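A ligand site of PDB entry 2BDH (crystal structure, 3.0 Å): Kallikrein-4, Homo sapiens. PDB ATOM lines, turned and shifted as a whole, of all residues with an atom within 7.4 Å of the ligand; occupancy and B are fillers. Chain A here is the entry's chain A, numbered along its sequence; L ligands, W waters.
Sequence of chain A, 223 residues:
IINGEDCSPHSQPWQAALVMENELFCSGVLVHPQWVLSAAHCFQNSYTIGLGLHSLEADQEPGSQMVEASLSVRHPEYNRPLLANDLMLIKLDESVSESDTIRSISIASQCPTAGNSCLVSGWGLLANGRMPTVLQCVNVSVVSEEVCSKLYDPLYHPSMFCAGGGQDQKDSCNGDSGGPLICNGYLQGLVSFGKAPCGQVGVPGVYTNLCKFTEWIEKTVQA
Water W2 lies within hydrogen-bond range of N3 of the ligand (2.9 Å), N of Gly 175 (3.0 Å) and OG of Ser 177 (3.2 Å).
Water W1 lies within hydrogen-bond range of the backbone carbonyl oxygen (O) of Val 206 (2.7 Å), the backbone carbonyl oxygen (O) of Phe 193 (2.8 Å) and a nitrogen (N2) of the ligand (2.9 Å).
The side-chain carboxylate (OD2) of Asp 171 lies within salt-bridge range of a nitrogen (N1) of the ligand (2.8 Å).
The side-chain hydroxyl (OG) of Ser 177 sits at hydrogen-bond distance from a nitrogen (N3) of the ligand (3.0 Å).
The backbone carbonyl oxygen (O) of Ser 172 lies close to a nitrogen (N2) of the ligand, at 3.1 Å.
The side-chain sulfur (SG) of Cys 198 sits at hydrogen-bond distance from a nitrogen (N1) of the ligand (3.5 Å).
Residues that only touch the ligand: Cys 173 (3.8 Å), Asn 174 (3.3 Å), Val 191 (3.6 Å), Ser 192 (3.8 Å), Phe 193 (3.7 Å) and Gly 194 (3.7 Å).
Hydrophobic or aromatic side chains that line the ligand: Val 191.
The nearest printed residue that does not touch the ligand is Gly 205 (4.04 Å).
The backbone carbonyl oxygen (O) of Asp 171 is in hydrogen-bond range of the backbone NH (N) of Ile 2 (2.9 Å).
The side-chain hydroxyl (OG) of Ser 177 lies within hydrogen-bond range of a ring nitrogen (NE2) of His 41, at 2.9 Å.
OG of Ser 172 lies within hydrogen-bond range of OH of Tyr 207 (3.0 Å).
The side-chain sulfur (SG) of Cys 198 is disulfide-bonded to the side-chain sulfur (SG) of Cys 173, 2.0 Å away.
The backbone carbonyl oxygen (O) of Val 191 sits at hydrogen-bond distance from the backbone NH (N) of Gly 178, 3.0 Å away.
The backbone NH of Val 206 sits at hydrogen-bond distance from the backbone carbonyl oxygen of Phe 193 (2.8 Å).
N of Ser 192 sits at hydrogen-bond distance from O of Val 206 (3.2 Å).
The backbone NH of Cys 173 is in hydrogen-bond range of the side-chain carboxylate of Asp 176 (3.1 Å).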
ATOM      1  N   ILE A   2      -1.833   5.727 -35.290  1.00  0.00           N
ATOM      2  CA  ILE A   2      -0.704   5.277 -36.105  1.00  0.00           C
ATOM      3  C   ILE A   2      -0.410   3.794 -35.905  1.00  0.00           C
ATOM      4  O   ILE A   2      -0.241   3.344 -34.777  1.00  0.00           O
ATOM      5  CB  ILE A   2       0.562   6.053 -35.751  1.00  0.00           C
ATOM      6  CG1 ILE A   2       0.202   7.482 -35.344  1.00  0.00           C
ATOM      7  CG2 ILE A   2       1.487   6.094 -36.913  1.00  0.00           C
ATOM      8  CD1 ILE A   2      -0.526   8.253 -36.374  1.00  0.00           C
ATOM      9  N   HIS A  41      -9.251  21.003 -25.092  1.00  0.00           N
ATOM     10  CA  HIS A  41      -8.880  21.732 -26.296  1.00  0.00           C
ATOM     11  C   HIS A  41      -9.818  21.439 -27.459  1.00  0.00           C
ATOM     12  O   HIS A  41      -9.574  21.858 -28.581  1.00  0.00           O
ATOM     13  CB  HIS A  41      -7.430  21.423 -26.696  1.00  0.00           C
ATOM     14  CG  HIS A  41      -7.221  20.060 -27.262  1.00  0.00           C
ATOM     15  ND1 HIS A  41      -7.119  18.930 -26.476  1.00  0.00           N
ATOM     16  CD2 HIS A  41      -7.045  19.643 -28.544  1.00  0.00           C
ATOM     17  CE1 HIS A  41      -6.900  17.877 -27.247  1.00  0.00           C
ATOM     18  NE2 HIS A  41      -6.853  18.281 -28.508  1.00  0.00           N
ATOM     19  N   TYR A 152       8.979  14.480 -20.567  1.00  0.00           N
ATOM     20  CA  TYR A 152       8.189  15.669 -20.916  1.00  0.00           C
ATOM     21  C   TYR A 152       8.405  16.872 -20.002  1.00  0.00           C
ATOM     22  O   TYR A 152       7.601  17.820 -20.030  1.00  0.00           O
ATOM     23  CB  TYR A 152       6.712  15.309 -20.926  1.00  0.00           C
ATOM     24  CG  TYR A 152       6.254  14.629 -22.181  1.00  0.00           C
ATOM     25  CD1 TYR A 152       5.928  15.366 -23.318  1.00  0.00           C
ATOM     26  CD2 TYR A 152       6.157  13.225 -22.259  1.00  0.00           C
ATOM     27  CE1 TYR A 152       5.514  14.758 -24.495  1.00  0.00           C
ATOM     28  CE2 TYR A 152       5.733  12.596 -23.439  1.00  0.00           C
ATOM     29  CZ  TYR A 152       5.413  13.376 -24.544  1.00  0.00           C
ATOM     30  OH  TYR A 152       4.980  12.804 -25.723  1.00  0.00           O
ATOM     31  N   ALA A 163       1.644   6.696 -22.495  1.00  0.00           N
ATOM     32  CA  ALA A 163       1.355   5.321 -22.914  1.00  0.00           C
ATOM     33  C   ALA A 163       1.953   5.136 -24.279  1.00  0.00           C
ATOM     34  O   ALA A 163       2.002   6.079 -25.064  1.00  0.00           O
ATOM     35  CB  ALA A 163      -0.106   5.083 -22.965  1.00  0.00           C
ATOM     36  N   ASP A 171       0.897   4.705 -31.760  1.00  0.00           N
ATOM     37  CA  ASP A 171       0.588   5.935 -31.029  1.00  0.00           C
ATOM     38  C   ASP A 171      -0.642   6.629 -31.544  1.00  0.00           C
ATOM     39  O   ASP A 171      -1.278   6.158 -32.467  1.00  0.00           O
ATOM     40  CB  ASP A 171       1.760   6.896 -31.142  1.00  0.00           C
ATOM     41  CG  ASP A 171       1.582   8.138 -30.295  1.00  0.00           C
ATOM     42  OD1 ASP A 171       1.135   8.015 -29.116  1.00  0.00           O
ATOM     43  OD2 ASP A 171       1.905   9.231 -30.832  1.00  0.00           O
ATOM     44  N   SER A 172      -0.994   7.751 -30.949  1.00  0.00           N
ATOM     45  CA  SER A 172      -2.165   8.490 -31.375  1.00  0.00           C
ATOM     46  C   SER A 172      -1.681   9.661 -32.224  1.00  0.00           C
ATOM     47  O   SER A 172      -0.475   9.853 -32.372  1.00  0.00           O
ATOM     48  CB  SER A 172      -2.908   9.034 -30.155  1.00  0.00           C
ATOM     49  OG  SER A 172      -3.149   8.023 -29.190  1.00  0.00           O
ATOM     50  N   CYS A 173      -2.610  10.429 -32.774  1.00  0.00           N
ATOM     51  CA  CYS A 173      -2.277  11.588 -33.605  1.00  0.00           C
ATOM     52  C   CYS A 173      -3.470  12.506 -33.816  1.00  0.00           C
ATOM     53  O   CYS A 173      -4.605  12.130 -33.534  1.00  0.00           O
ATOM     54  CB  CYS A 173      -1.725  11.140 -34.956  1.00  0.00           C
ATOM     55  SG  CYS A 173      -0.278  12.123 -35.480  1.00  0.00           S
ATOM     56  N   ASN A 174      -3.193  13.703 -34.317  1.00  0.00           N
ATOM     57  CA  ASN A 174      -4.212  14.718 -34.580  1.00  0.00           C
ATOM     58  C   ASN A 174      -5.506  14.054 -35.023  1.00  0.00           C
ATOM     59  O   ASN A 174      -5.483  13.140 -35.857  1.00  0.00           O
ATOM     60  CB  ASN A 174      -3.736  15.661 -35.679  1.00  0.00           C
ATOM     61  CG  ASN A 174      -2.258  15.975 -35.575  1.00  0.00           C
ATOM     62  OD1 ASN A 174      -1.473  15.699 -36.489  1.00  0.00           O
ATOM     63  ND2 ASN A 174      -1.854  16.552 -34.442  1.00  0.00           N
ATOM     64  N   GLY A 175      -6.624  14.502 -34.446  1.00  0.00           N
ATOM     65  CA  GLY A 175      -7.926  13.956 -34.782  1.00  0.00           C
ATOM     66  C   GLY A 175      -8.369  12.879 -33.826  1.00  0.00           C
ATOM     67  O   GLY A 175      -9.536  12.491 -33.777  1.00  0.00           O
ATOM     68  N   ASP A 176      -7.423  12.362 -33.055  1.00  0.00           N
ATOM     69  CA  ASP A 176      -7.755  11.340 -32.091  1.00  0.00           C
ATOM     70  C   ASP A 176      -8.023  11.990 -30.753  1.00  0.00           C
ATOM     71  O   ASP A 176      -8.495  11.351 -29.824  1.00  0.00           O
ATOM     72  CB  ASP A 176      -6.605  10.351 -31.949  1.00  0.00           C
ATOM     73  CG  ASP A 176      -6.495   9.412 -33.115  1.00  0.00           C
ATOM     74  OD1 ASP A 176      -7.496   8.755 -33.469  1.00  0.00           O
ATOM     75  OD2 ASP A 176      -5.381   9.315 -33.678  1.00  0.00           O
ATOM     76  N   SER A 177      -7.710  13.287 -30.657  1.00  0.00           N
ATOM     77  CA  SER A 177      -7.891  14.016 -29.405  1.00  0.00           C
ATOM     78  C   SER A 177      -9.245  13.764 -28.802  1.00  0.00           C
ATOM     79  O   SER A 177     -10.240  13.789 -29.511  1.00  0.00           O
ATOM     80  CB  SER A 177      -7.711  15.522 -29.640  1.00  0.00           C
ATOM     81  OG  SER A 177      -6.350  15.824 -29.881  1.00  0.00           O
ATOM     82  N   GLY A 178      -9.283  13.508 -27.489  1.00  0.00           N
ATOM     83  CA  GLY A 178     -10.522  13.255 -26.795  1.00  0.00           C
ATOM     84  C   GLY A 178     -10.873  11.791 -26.835  1.00  0.00           C
ATOM     85  O   GLY A 178     -11.703  11.291 -26.068  1.00  0.00           O
ATOM     86  N   VAL A 191      -7.147  10.899 -25.147  1.00  0.00           N
ATOM     87  CA  VAL A 191      -6.035  11.380 -25.977  1.00  0.00           C
ATOM     88  C   VAL A 191      -5.823  12.883 -25.720  1.00  0.00           C
ATOM     89  O   VAL A 191      -6.732  13.687 -25.931  1.00  0.00           O
ATOM     90  CB  VAL A 191      -6.337  11.135 -27.465  1.00  0.00           C
ATOM     91  CG1 VAL A 191      -5.118  11.392 -28.304  1.00  0.00           C
ATOM     92  CG2 VAL A 191      -6.806   9.738 -27.652  1.00  0.00           C
ATOM     93  N   SER A 192      -4.624  13.257 -25.295  1.00  0.00           N
ATOM     94  CA  SER A 192      -4.315  14.657 -24.994  1.00  0.00           C
ATOM     95  C   SER A 192      -3.315  15.299 -25.939  1.00  0.00           C
ATOM     96  O   SER A 192      -3.657  16.233 -26.642  1.00  0.00           O
ATOM     97  CB  SER A 192      -3.785  14.784 -23.574  1.00  0.00           C
ATOM     98  OG  SER A 192      -3.506  16.145 -23.288  1.00  0.00           O
ATOM     99  N   PHE A 193      -2.078  14.824 -25.918  1.00  0.00           N
ATOM    100  CA  PHE A 193      -1.067  15.368 -26.814  1.00  0.00           C
ATOM    101  C   PHE A 193       0.159  14.472 -26.929  1.00  0.00           C
ATOM    102  O   PHE A 193       0.153  13.324 -26.479  1.00  0.00           O
ATOM    103  CB  PHE A 193      -0.656  16.778 -26.345  1.00  0.00           C
ATOM    104  CG  PHE A 193       0.205  16.778 -25.141  1.00  0.00           C
ATOM    105  CD1 PHE A 193       1.569  16.668 -25.245  1.00  0.00           C
ATOM    106  CD2 PHE A 193      -0.361  16.866 -23.883  1.00  0.00           C
ATOM    107  CE1 PHE A 193       2.366  16.647 -24.123  1.00  0.00           C
ATOM    108  CE2 PHE A 193       0.436  16.844 -22.761  1.00  0.00           C
ATOM    109  CZ  PHE A 193       1.795  16.731 -22.884  1.00  0.00           C
ATOM    110  N   GLY A 194       1.200  14.999 -27.564  1.00  0.00           N
ATOM    111  CA  GLY A 194       2.424  14.249 -27.739  1.00  0.00           C
ATOM    112  C   GLY A 194       3.300  14.936 -28.772  1.00  0.00           C
ATOM    113  O   GLY A 194       2.792  15.672 -29.617  1.00  0.00           O
ATOM    114  N   LYS A 195       4.604  14.686 -28.701  1.00  0.00           N
ATOM    115  CA  LYS A 195       5.565  15.257 -29.651  1.00  0.00           C
ATOM    116  C   LYS A 195       5.273  14.806 -31.079  1.00  0.00           C
ATOM    117  O   LYS A 195       4.895  13.661 -31.325  1.00  0.00           O
ATOM    118  CB  LYS A 195       7.000  14.863 -29.281  1.00  0.00           C
ATOM    119  CG  LYS A 195       7.427  15.285 -27.889  1.00  0.00           C
ATOM    120  CD  LYS A 195       8.857  14.836 -27.539  1.00  0.00           C
ATOM    121  CE  LYS A 195       9.141  14.945 -26.017  1.00  0.00           C
ATOM    122  NZ  LYS A 195      10.512  14.445 -25.649  1.00  0.00           N
ATOM    123  N   ALA A 196       5.470  15.713 -32.030  1.00  0.00           N
ATOM    124  CA  ALA A 196       5.231  15.398 -33.428  1.00  0.00           C
ATOM    125  C   ALA A 196       6.574  15.253 -34.127  1.00  0.00           C
ATOM    126  O   ALA A 196       7.557  15.905 -33.734  1.00  0.00           O
ATOM    127  CB  ALA A 196       4.411  16.489 -34.100  1.00  0.00           C
ATOM    128  N   PRO A 197       6.645  14.377 -35.144  1.00  0.00           N
ATOM    129  CA  PRO A 197       5.522  13.559 -35.630  1.00  0.00           C
ATOM    130  C   PRO A 197       5.163  12.422 -34.667  1.00  0.00           C
ATOM    131  O   PRO A 197       5.908  12.106 -33.746  1.00  0.00           O
ATOM    132  CB  PRO A 197       6.047  13.022 -36.965  1.00  0.00           C
ATOM    133  CG  PRO A 197       7.502  12.820 -36.673  1.00  0.00           C
ATOM    134  CD  PRO A 197       7.862  14.104 -35.927  1.00  0.00           C
ATOM    135  N   CYS A 198       4.007  11.811 -34.907  1.00  0.00           N
ATOM    136  CA  CYS A 198       3.546  10.714 -34.080  1.00  0.00           C
ATOM    137  C   CYS A 198       4.284   9.430 -34.411  1.00  0.00           C
ATOM    138  O   CYS A 198       4.799   9.277 -35.512  1.00  0.00           O
ATOM    139  CB  CYS A 198       2.055  10.499 -34.297  1.00  0.00           C
ATOM    140  SG  CYS A 198       1.037  11.963 -33.926  1.00  0.00           S
ATOM    141  N   GLY A 199       4.313   8.505 -33.463  1.00  0.00           N
ATOM    142  CA  GLY A 199       4.969   7.225 -33.694  1.00  0.00           C
ATOM    143  C   GLY A 199       6.482   7.243 -33.615  1.00  0.00           C
ATOM    144  O   GLY A 199       7.130   6.511 -34.351  1.00  0.00           O
ATOM    145  N   GLN A 200       7.037   8.054 -32.737  1.00  0.00           N
ATOM    146  CA  GLN A 200       8.488   8.134 -32.587  1.00  0.00           C
ATOM    147  C   GLN A 200       8.907   7.177 -31.508  1.00  0.00           C
ATOM    148  O   GLN A 200       8.354   7.193 -30.411  1.00  0.00           O
ATOM    149  CB  GLN A 200       8.942   9.530 -32.171  1.00  0.00           C
ATOM    150  CG  GLN A 200       8.445  10.646 -33.065  1.00  0.00           C
ATOM    151  CD  GLN A 200       8.877  12.019 -32.563  1.00  0.00           C
ATOM    152  OE1 GLN A 200       8.354  13.046 -33.004  1.00  0.00           O
ATOM    153  NE2 GLN A 200       9.839  12.032 -31.649  1.00  0.00           N
ATOM    154  N   VAL A 203       9.077   7.978 -27.595  1.00  0.00           N
ATOM    155  CA  VAL A 203       8.270   9.152 -27.284  1.00  0.00           C
ATOM    156  C   VAL A 203       6.800   8.791 -27.168  1.00  0.00           C
ATOM    157  O   VAL A 203       6.018   8.946 -28.108  1.00  0.00           O
ATOM    158  CB  VAL A 203       8.416  10.220 -28.369  1.00  0.00           C
ATOM    159  CG1 VAL A 203       7.788  11.485 -27.909  1.00  0.00           C
ATOM    160  CG2 VAL A 203       9.876  10.441 -28.699  1.00  0.00           C
ATOM    161  N   PRO A 204       6.392   8.309 -26.003  1.00  0.00           N
ATOM    162  CA  PRO A 204       5.002   7.917 -25.777  1.00  0.00           C
ATOM    163  C   PRO A 204       4.053   9.109 -25.810  1.00  0.00           C
ATOM    164  O   PRO A 204       4.468  10.232 -25.529  1.00  0.00           O
ATOM    165  CB  PRO A 204       5.066   7.246 -24.422  1.00  0.00           C
ATOM    166  CG  PRO A 204       6.120   8.033 -23.727  1.00  0.00           C
ATOM    167  CD  PRO A 204       7.178   8.114 -24.778  1.00  0.00           C
ATOM    168  N   GLY A 205       2.790   8.859 -26.144  1.00  0.00           N
ATOM    169  CA  GLY A 205       1.807   9.919 -26.193  1.00  0.00           C
ATOM    170  C   GLY A 205       1.247  10.173 -24.800  1.00  0.00           C
ATOM    171  O   GLY A 205       1.203   9.260 -23.981  1.00  0.00           O
ATOM    172  N   VAL A 206       0.809  11.400 -24.540  1.00  0.00           N
ATOM    173  CA  VAL A 206       0.282  11.753 -23.221  1.00  0.00           C
ATOM    174  C   VAL A 206      -1.247  11.732 -23.252  1.00  0.00           C
ATOM    175  O   VAL A 206      -1.862  12.098 -24.255  1.00  0.00           O
ATOM    176  CB  VAL A 206       0.774  13.180 -22.759  1.00  0.00           C
ATOM    177  CG1 VAL A 206       0.629  13.322 -21.269  1.00  0.00           C
ATOM    178  CG2 VAL A 206       2.211  13.425 -23.150  1.00  0.00           C
ATOM    179  N   TYR A 207      -1.857  11.318 -22.144  1.00  0.00           N
ATOM    180  CA  TYR A 207      -3.311  11.235 -22.047  1.00  0.00           C
ATOM    181  C   TYR A 207      -3.756  11.882 -20.760  1.00  0.00           C
ATOM    182  O   TYR A 207      -2.936  12.104 -19.876  1.00  0.00           O
ATOM    183  CB  TYR A 207      -3.742   9.766 -22.029  1.00  0.00           C
ATOM    184  CG  TYR A 207      -3.288   8.990 -23.240  1.00  0.00           C
ATOM    185  CD1 TYR A 207      -2.005   8.480 -23.301  1.00  0.00           C
ATOM    186  CD2 TYR A 207      -4.128   8.804 -24.359  1.00  0.00           C
ATOM    187  CE1 TYR A 207      -1.548   7.794 -24.435  1.00  0.00           C
ATOM    188  CE2 TYR A 207      -3.674   8.105 -25.521  1.00  0.00           C
ATOM    189  CZ  TYR A 207      -2.366   7.601 -25.549  1.00  0.00           C
ATOM    190  OH  TYR A 207      -1.854   6.962 -26.688  1.00  0.00           O
HETATM  191  N1  LIG L   1       1.252  11.976 -30.463  1.00  0.00           N
HETATM  192  N2  LIG L   1      -0.461  10.853 -29.401  1.00  0.00           N
HETATM  193  C1  LIG L   1      -0.014  11.902 -30.053  1.00  0.00           C
HETATM  194  C2  LIG L   1      -0.972  13.085 -30.295  1.00  0.00           C
HETATM  195  C3  LIG L   1      -3.085  14.256 -29.789  1.00  0.00           C
HETATM  196  C4  LIG L   1      -2.198  13.171 -29.578  1.00  0.00           C
HETATM  197  C5  LIG L   1      -0.642  14.105 -31.236  1.00  0.00           C
HETATM  198  C6  LIG L   1      -1.532  15.200 -31.438  1.00  0.00           C
HETATM  199  C7  LIG L   1      -2.745  15.270 -30.722  1.00  0.00           C
HETATM  200  N3  LIG L   1      -3.612  16.358 -30.919  1.00  0.00           N
HETATM  201  O   HOH W   1      -1.526  11.140 -26.726  1.00  0.00           O
HETATM  202  O   HOH W   2      -5.654  16.909 -32.849  1.00  0.00           O
